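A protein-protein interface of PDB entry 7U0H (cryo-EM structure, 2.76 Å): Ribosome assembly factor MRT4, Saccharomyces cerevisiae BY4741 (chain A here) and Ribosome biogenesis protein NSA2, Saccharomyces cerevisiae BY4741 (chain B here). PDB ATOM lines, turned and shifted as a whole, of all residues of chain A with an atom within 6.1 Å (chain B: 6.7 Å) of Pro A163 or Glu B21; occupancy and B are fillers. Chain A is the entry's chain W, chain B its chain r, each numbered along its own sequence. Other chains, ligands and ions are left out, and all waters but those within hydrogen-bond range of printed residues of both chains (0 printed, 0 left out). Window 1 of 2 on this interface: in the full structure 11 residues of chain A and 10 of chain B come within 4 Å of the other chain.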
ATOM      1  N   HIS A 159       8.993  29.433  29.614  1.00  0.00           N
ATOM      2  CA  HIS A 159       9.503  28.163  29.111  1.00  0.00           C
ATOM      3  C   HIS A 159      11.006  28.019  29.311  1.00  0.00           C
ATOM      4  O   HIS A 159      11.519  26.896  29.267  1.00  0.00           O
ATOM      5  CB  HIS A 159       9.167  28.014  27.629  1.00  0.00           C
ATOM      6  CG  HIS A 159       9.681  29.134  26.781  1.00  0.00           C
ATOM      7  ND1 HIS A 159       9.012  30.332  26.648  1.00  0.00           N
ATOM      8  CD2 HIS A 159      10.802  29.245  26.032  1.00  0.00           C
ATOM      9  CE1 HIS A 159       9.699  31.130  25.852  1.00  0.00           C
ATOM     10  NE2 HIS A 159      10.788  30.495  25.462  1.00  0.00           N
ATOM     11  N   SER A 160      11.720  29.124  29.526  1.00  0.00           N
ATOM     12  CA  SER A 160      13.174  29.076  29.624  1.00  0.00           C
ATOM     13  C   SER A 160      13.650  28.461  30.929  1.00  0.00           C
ATOM     14  O   SER A 160      14.797  28.013  31.004  1.00  0.00           O
ATOM     15  CB  SER A 160      13.754  30.479  29.474  1.00  0.00           C
ATOM     16  OG  SER A 160      13.282  31.098  28.291  1.00  0.00           O
ATOM     17  N   LEU A 161      12.806  28.428  31.954  1.00  0.00           N
ATOM     18  CA  LEU A 161      13.186  27.889  33.251  1.00  0.00           C
ATOM     19  C   LEU A 161      12.844  26.416  33.404  1.00  0.00           C
ATOM     20  O   LEU A 161      13.189  25.818  34.427  1.00  0.00           O
ATOM     21  CB  LEU A 161      12.517  28.693  34.369  1.00  0.00           C
ATOM     22  CG  LEU A 161      13.315  29.858  34.957  1.00  0.00           C
ATOM     23  CD1 LEU A 161      13.893  30.745  33.872  1.00  0.00           C
ATOM     24  CD2 LEU A 161      12.433  30.669  35.879  1.00  0.00           C
ATOM     25  N   GLU A 162      12.170  25.822  32.421  1.00  0.00           N
ATOM     26  CA  GLU A 162      11.797  24.414  32.525  1.00  0.00           C
ATOM     27  C   GLU A 162      13.002  23.484  32.605  1.00  0.00           C
ATOM     28  O   GLU A 162      12.980  22.559  33.435  1.00  0.00           O
ATOM     29  CB  GLU A 162      10.867  24.042  31.366  1.00  0.00           C
ATOM     30  CG  GLU A 162      10.117  22.740  31.573  1.00  0.00           C
ATOM     31  CD  GLU A 162      10.947  21.526  31.218  1.00  0.00           C
ATOM     32  OE1 GLU A 162      11.480  21.477  30.089  1.00  0.00           O
ATOM     33  OE2 GLU A 162      11.076  20.626  32.073  1.00  0.00           O
ATOM     34  N   PRO A 163      14.052  23.629  31.783  1.00  0.00           N
ATOM     35  CA  PRO A 163      15.230  22.765  31.976  1.00  0.00           C
ATOM     36  C   PRO A 163      15.856  22.890  33.353  1.00  0.00           C
ATOM     37  O   PRO A 163      16.267  21.878  33.934  1.00  0.00           O
ATOM     38  CB  PRO A 163      16.189  23.236  30.876  1.00  0.00           C
ATOM     39  CG  PRO A 163      15.314  23.801  29.837  1.00  0.00           C
ATOM     40  CD  PRO A 163      14.182  24.447  30.563  1.00  0.00           C
ATOM     41  N   THR A 164      15.931  24.106  33.899  1.00  0.00           N
ATOM     42  CA  THR A 164      16.531  24.293  35.217  1.00  0.00           C
ATOM     43  C   THR A 164      15.727  23.570  36.288  1.00  0.00           C
ATOM     44  O   THR A 164      16.287  22.885  37.151  1.00  0.00           O
ATOM     45  CB  THR A 164      16.634  25.783  35.542  1.00  0.00           C
ATOM     46  OG1 THR A 164      17.281  26.469  34.462  1.00  0.00           O
ATOM     47  CG2 THR A 164      17.431  25.993  36.814  1.00  0.00           C
ATOM     48  N   MET A 165      14.402  23.706  36.237  1.00  0.00           N
ATOM     49  CA  MET A 165      13.541  23.028  37.196  1.00  0.00           C
ATOM     50  C   MET A 165      13.617  21.518  37.037  1.00  0.00           C
ATOM     51  O   MET A 165      13.623  20.779  38.028  1.00  0.00           O
ATOM     52  CB  MET A 165      12.106  23.513  37.025  1.00  0.00           C
ATOM     53  CG  MET A 165      11.286  23.452  38.287  1.00  0.00           C
ATOM     54  SD  MET A 165       9.886  24.578  38.212  1.00  0.00           S
ATOM     55  CE  MET A 165       9.363  24.545  39.919  1.00  0.00           C
ATOM     56  N   ARG A 166      13.683  21.042  35.795  1.00  0.00           N
ATOM     57  CA  ARG A 166      13.706  19.607  35.547  1.00  0.00           C
ATOM     58  C   ARG A 166      15.027  18.980  35.970  1.00  0.00           C
ATOM     59  O   ARG A 166      15.049  17.823  36.401  1.00  0.00           O
ATOM     60  CB  ARG A 166      13.429  19.340  34.068  1.00  0.00           C
ATOM     61  CG  ARG A 166      13.368  17.877  33.687  1.00  0.00           C
ATOM     62  CD  ARG A 166      12.612  17.693  32.387  1.00  0.00           C
ATOM     63  NE  ARG A 166      12.899  18.755  31.427  1.00  0.00           N
ATOM     64  CZ  ARG A 166      13.969  18.790  30.646  1.00  0.00           C
ATOM     65  NH1 ARG A 166      14.889  17.842  30.692  1.00  0.00           N
ATOM     66  NH2 ARG A 166      14.122  19.805  29.801  1.00  0.00           N
ATOM     67  N   ASN A 167      16.130  19.719  35.863  1.00  0.00           N
ATOM     68  CA  ASN A 167      17.438  19.150  36.161  1.00  0.00           C
ATOM     69  C   ASN A 167      17.887  19.437  37.593  1.00  0.00           C
ATOM     70  O   ASN A 167      18.086  18.506  38.380  1.00  0.00           O
ATOM     71  CB  ASN A 167      18.465  19.669  35.148  1.00  0.00           C
ATOM     72  CG  ASN A 167      18.149  19.231  33.730  1.00  0.00           C
ATOM     73  OD1 ASN A 167      17.521  18.194  33.518  1.00  0.00           O
ATOM     74  ND2 ASN A 167      18.578  20.019  32.751  1.00  0.00           N
ATOM     75  N   LYS A 168      18.047  20.714  37.949  1.00  0.00           N
ATOM     76  CA  LYS A 168      18.589  21.032  39.268  1.00  0.00           C
ATOM     77  C   LYS A 168      17.551  20.869  40.372  1.00  0.00           C
ATOM     78  O   LYS A 168      17.878  20.395  41.465  1.00  0.00           O
ATOM     79  CB  LYS A 168      19.157  22.450  39.288  1.00  0.00           C
ATOM     80  CG  LYS A 168      19.905  22.779  40.573  1.00  0.00           C
ATOM     81  CD  LYS A 168      20.895  23.912  40.374  1.00  0.00           C
ATOM     82  CE  LYS A 168      21.845  24.034  41.555  1.00  0.00           C
ATOM     83  NZ  LYS A 168      22.564  22.763  41.827  1.00  0.00           N
ATOM     84  N   THR A 173       8.844  17.930  35.118  1.00  0.00           N
ATOM     85  CA  THR A 173       8.190  19.026  34.426  1.00  0.00           C
ATOM     86  C   THR A 173       8.171  18.738  32.935  1.00  0.00           C
ATOM     87  O   THR A 173       9.116  18.157  32.393  1.00  0.00           O
ATOM     88  CB  THR A 173       8.901  20.358  34.686  1.00  0.00           C
ATOM     89  OG1 THR A 173      10.313  20.185  34.518  1.00  0.00           O
ATOM     90  CG2 THR A 173       8.616  20.854  36.095  1.00  0.00           C
ATOM     91  N   ILE A 175       6.760  20.641  29.046  1.00  0.00           N
ATOM     92  CA  ILE A 175       6.296  21.841  28.364  1.00  0.00           C
ATOM     93  C   ILE A 175       5.158  21.447  27.432  1.00  0.00           C
ATOM     94  O   ILE A 175       5.345  20.637  26.517  1.00  0.00           O
ATOM     95  CB  ILE A 175       7.432  22.533  27.598  1.00  0.00           C
ATOM     96  CG1 ILE A 175       8.309  23.329  28.561  1.00  0.00           C
ATOM     97  CG2 ILE A 175       6.878  23.453  26.529  1.00  0.00           C
ATOM     98  CD1 ILE A 175       9.267  24.282  27.873  1.00  0.00           C
ATOM     99  N   LYS B  16      13.289  21.321  23.900  1.00  0.00           N
ATOM    100  CA  LYS B  16      14.277  20.536  23.176  1.00  0.00           C
ATOM    101  C   LYS B  16      14.243  19.097  23.682  1.00  0.00           C
ATOM    102  O   LYS B  16      13.378  18.714  24.471  1.00  0.00           O
ATOM    103  CB  LYS B  16      15.665  21.162  23.326  1.00  0.00           C
ATOM    104  CG  LYS B  16      15.709  22.637  22.974  1.00  0.00           C
ATOM    105  CD  LYS B  16      17.043  23.277  23.323  1.00  0.00           C
ATOM    106  CE  LYS B  16      16.956  24.793  23.238  1.00  0.00           C
ATOM    107  NZ  LYS B  16      18.251  25.461  23.539  1.00  0.00           N
ATOM    108  N   ARG B  17      15.184  18.287  23.201  1.00  0.00           N
ATOM    109  CA  ARG B  17      15.321  16.934  23.721  1.00  0.00           C
ATOM    110  C   ARG B  17      15.737  16.988  25.186  1.00  0.00           C
ATOM    111  O   ARG B  17      16.420  17.916  25.625  1.00  0.00           O
ATOM    112  CB  ARG B  17      16.337  16.138  22.899  1.00  0.00           C
ATOM    113  CG  ARG B  17      15.829  15.731  21.520  1.00  0.00           C
ATOM    114  CD  ARG B  17      16.946  15.212  20.635  1.00  0.00           C
ATOM    115  NE  ARG B  17      17.576  14.017  21.179  1.00  0.00           N
ATOM    116  CZ  ARG B  17      17.288  12.781  20.802  1.00  0.00           C
ATOM    117  NH1 ARG B  17      16.378  12.535  19.875  1.00  0.00           N
ATOM    118  NH2 ARG B  17      17.926  11.764  21.373  1.00  0.00           N
ATOM    119  N   LEU B  18      15.309  15.982  25.952  1.00  0.00           N
ATOM    120  CA  LEU B  18      15.416  16.071  27.404  1.00  0.00           C
ATOM    121  C   LEU B  18      16.861  16.155  27.877  1.00  0.00           C
ATOM    122  O   LEU B  18      17.118  16.652  28.978  1.00  0.00           O
ATOM    123  CB  LEU B  18      14.709  14.885  28.059  1.00  0.00           C
ATOM    124  CG  LEU B  18      13.188  14.876  27.896  1.00  0.00           C
ATOM    125  CD1 LEU B  18      12.548  13.871  28.835  1.00  0.00           C
ATOM    126  CD2 LEU B  18      12.605  16.263  28.125  1.00  0.00           C
ATOM    127  N   ASP B  19      17.813  15.684  27.070  1.00  0.00           N
ATOM    128  CA  ASP B  19      19.222  15.674  27.444  1.00  0.00           C
ATOM    129  C   ASP B  19      20.050  16.677  26.646  1.00  0.00           C
ATOM    130  O   ASP B  19      21.275  16.541  26.578  1.00  0.00           O
ATOM    131  CB  ASP B  19      19.801  14.267  27.284  1.00  0.00           C
ATOM    132  CG  ASP B  19      19.746  13.767  25.854  1.00  0.00           C
ATOM    133  OD1 ASP B  19      19.183  14.467  24.985  1.00  0.00           O
ATOM    134  OD2 ASP B  19      20.268  12.664  25.595  1.00  0.00           O
ATOM    135  N   HIS B  20      19.410  17.675  26.039  1.00  0.00           N
ATOM    136  CA  HIS B  20      20.125  18.588  25.151  1.00  0.00           C
ATOM    137  C   HIS B  20      21.193  19.378  25.903  1.00  0.00           C
ATOM    138  O   HIS B  20      22.337  19.496  25.440  1.00  0.00           O
ATOM    139  CB  HIS B  20      19.134  19.527  24.467  1.00  0.00           C
ATOM    140  CG  HIS B  20      19.780  20.537  23.570  1.00  0.00           C
ATOM    141  ND1 HIS B  20      20.107  21.805  23.996  1.00  0.00           N
ATOM    142  CD2 HIS B  20      20.169  20.463  22.277  1.00  0.00           C
ATOM    143  CE1 HIS B  20      20.671  22.469  23.003  1.00  0.00           C
ATOM    144  NE2 HIS B  20      20.720  21.678  21.948  1.00  0.00           N
ATOM    145  N   GLU B  21      20.840  19.917  27.074  1.00  0.00           N
ATOM    146  CA  GLU B  21      21.769  20.761  27.820  1.00  0.00           C
ATOM    147  C   GLU B  21      22.993  19.974  28.273  1.00  0.00           C
ATOM    148  O   GLU B  21      24.134  20.390  28.040  1.00  0.00           O
ATOM    149  CB  GLU B  21      21.069  21.382  29.033  1.00  0.00           C
ATOM    150  CG  GLU B  21      19.820  22.176  28.725  1.00  0.00           C
ATOM    151  CD  GLU B  21      18.607  21.296  28.516  1.00  0.00           C
ATOM    152  OE1 GLU B  21      18.567  20.190  29.095  1.00  0.00           O
ATOM    153  OE2 GLU B  21      17.697  21.707  27.763  1.00  0.00           O
ATOM    154  N   GLU B  22      22.770  18.838  28.933  1.00  0.00           N
ATOM    155  CA  GLU B  22      23.884  18.039  29.424  1.00  0.00           C
ATOM    156  C   GLU B  22      24.711  17.476  28.278  1.00  0.00           C
ATOM    157  O   GLU B  22      25.935  17.362  28.399  1.00  0.00           O
ATOM    158  CB  GLU B  22      23.380  16.920  30.334  1.00  0.00           C
ATOM    159  CG  GLU B  22      22.115  16.223  29.865  1.00  0.00           C
ATOM    160  CD  GLU B  22      20.845  16.898  30.367  1.00  0.00           C
ATOM    161  OE1 GLU B  22      20.790  18.147  30.363  1.00  0.00           O
ATOM    162  OE2 GLU B  22      19.905  16.178  30.773  1.00  0.00           O
ATOM    163  N   ARG B  23      24.070  17.145  27.158  1.00  0.00           N
ATOM    164  CA  ARG B  23      24.809  16.678  25.992  1.00  0.00           C
ATOM    165  C   ARG B  23      25.765  17.752  25.488  1.00  0.00           C
ATOM    166  O   ARG B  23      26.956  17.489  25.265  1.00  0.00           O
ATOM    167  CB  ARG B  23      23.821  16.262  24.904  1.00  0.00           C
ATOM    168  CG  ARG B  23      24.375  15.332  23.850  1.00  0.00           C
ATOM    169  CD  ARG B  23      23.251  14.538  23.216  1.00  0.00           C
ATOM    170  NE  ARG B  23      23.634  13.963  21.932  1.00  0.00           N
ATOM    171  CZ  ARG B  23      24.133  12.745  21.774  1.00  0.00           C
ATOM    172  NH1 ARG B  23      24.333  11.941  22.804  1.00  0.00           N
ATOM    173  NH2 ARG B  23      24.436  12.324  20.549  1.00  0.00           N
ATOM    174  N   LYS B  24      25.265  18.981  25.325  1.00  0.00           N
ATOM    175  CA  LYS B  24      26.127  20.068  24.871  1.00  0.00           C
ATOM    176  C   LYS B  24      27.247  20.340  25.870  1.00  0.00           C
ATOM    177  O   LYS B  24      28.402  20.561  25.478  1.00  0.00           O
ATOM    178  CB  LYS B  24      25.297  21.331  24.636  1.00  0.00           C
ATOM    179  CG  LYS B  24      26.085  22.489  24.050  1.00  0.00           C
ATOM    180  CD  LYS B  24      25.349  23.809  24.208  1.00  0.00           C
ATOM    181  CE  LYS B  24      24.052  23.829  23.419  1.00  0.00           C
ATOM    182  NZ  LYS B  24      24.278  23.677  21.954  1.00  0.00           N
ATOM    183  N   ARG B  25      26.924  20.320  27.165  1.00  0.00           N
ATOM    184  CA  ARG B  25      27.922  20.618  28.187  1.00  0.00           C
ATOM    185  C   ARG B  25      29.042  19.587  28.184  1.00  0.00           C
ATOM    186  O   ARG B  25      30.226  19.942  28.213  1.00  0.00           O
ATOM    187  CB  ARG B  25      27.262  20.683  29.562  1.00  0.00           C
ATOM    188  CG  ARG B  25      28.249  20.922  30.687  1.00  0.00           C
ATOM    189  CD  ARG B  25      27.640  20.677  32.051  1.00  0.00           C
ATOM    190  NE  ARG B  25      27.301  19.275  32.267  1.00  0.00           N
ATOM    191  CZ  ARG B  25      28.146  18.356  32.712  1.00  0.00           C
ATOM    192  NH1 ARG B  25      29.407  18.647  32.983  1.00  0.00           N
ATOM    193  NH2 ARG B  25      27.719  17.110  32.881  1.00  0.00           N
ATOM    194  N   LYS B  26      28.689  18.299  28.152  1.00  0.00           N
ATOM    195  CA  LYS B  26      29.714  17.262  28.150  1.00  0.00           C
ATOM    196  C   LYS B  26      30.529  17.305  26.867  1.00  0.00           C
ATOM    197  O   LYS B  26      31.746  17.086  26.895  1.00  0.00           O
ATOM    198  CB  LYS B  26      29.082  15.885  28.350  1.00  0.00           C
ATOM    199  CG  LYS B  26      28.309  15.744  29.647  1.00  0.00           C
ATOM    200  CD  LYS B  26      27.900  14.315  29.905  1.00  0.00           C
ATOM    201  CE  LYS B  26      29.037  13.530  30.542  1.00  0.00           C
ATOM    202  NZ  LYS B  26      28.611  12.171  30.955  1.00  0.00           N
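Of the printed residues of chain A, Glu B21 touches Pro A163 and Asn A167.
Of the printed residues of chain A, Leu B18 touches Arg A166.
Printed residues of chain B within 4 Å of Arg A166: Leu B18.
Of the printed residues of chain B, Asn A167 touches Glu B21 and Glu B22.
The nearest residue of chain A that does not touch Glu B21 is Arg A166 (4.5 Å).
Among the printed residues, pairs that only touch across the chains: Pro A163 with Glu B21 (3.8 Å), Asn A167 with Glu B21 (3.7 Å) and Asn A167 with Glu B22 (3.8 Å).
NE of Arg A166 is in salt-bridge range of OE2 of Glu A162, 2.7 Å away.
The side-chain amide nitrogen of Asn A167 lies within hydrogen-bond range of the backbone carbonyl oxygen of Pro A163, at 3.2 Å.
Hydrophobic or aromatic side chains of chain B within 4 Å of the printed part of chain A: Leu B18.
Printed residues of chain A that touch a printed residue of chain B: Pro A163, Arg A166 and Asn A167.
Hydrophobic or aromatic side chains of chain A that line the printed part of chain B: Pro A163.
Among the printed residues, no Asp or Glu carboxylate lies within 4 Å of a Lys or Arg side-chain nitrogen of the other chain.
The guanidinium group (NH1) of Arg A166 is in hydrogen-bond range of the backbone carbonyl oxygen (O) of Leu B18 (3.1 Å).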
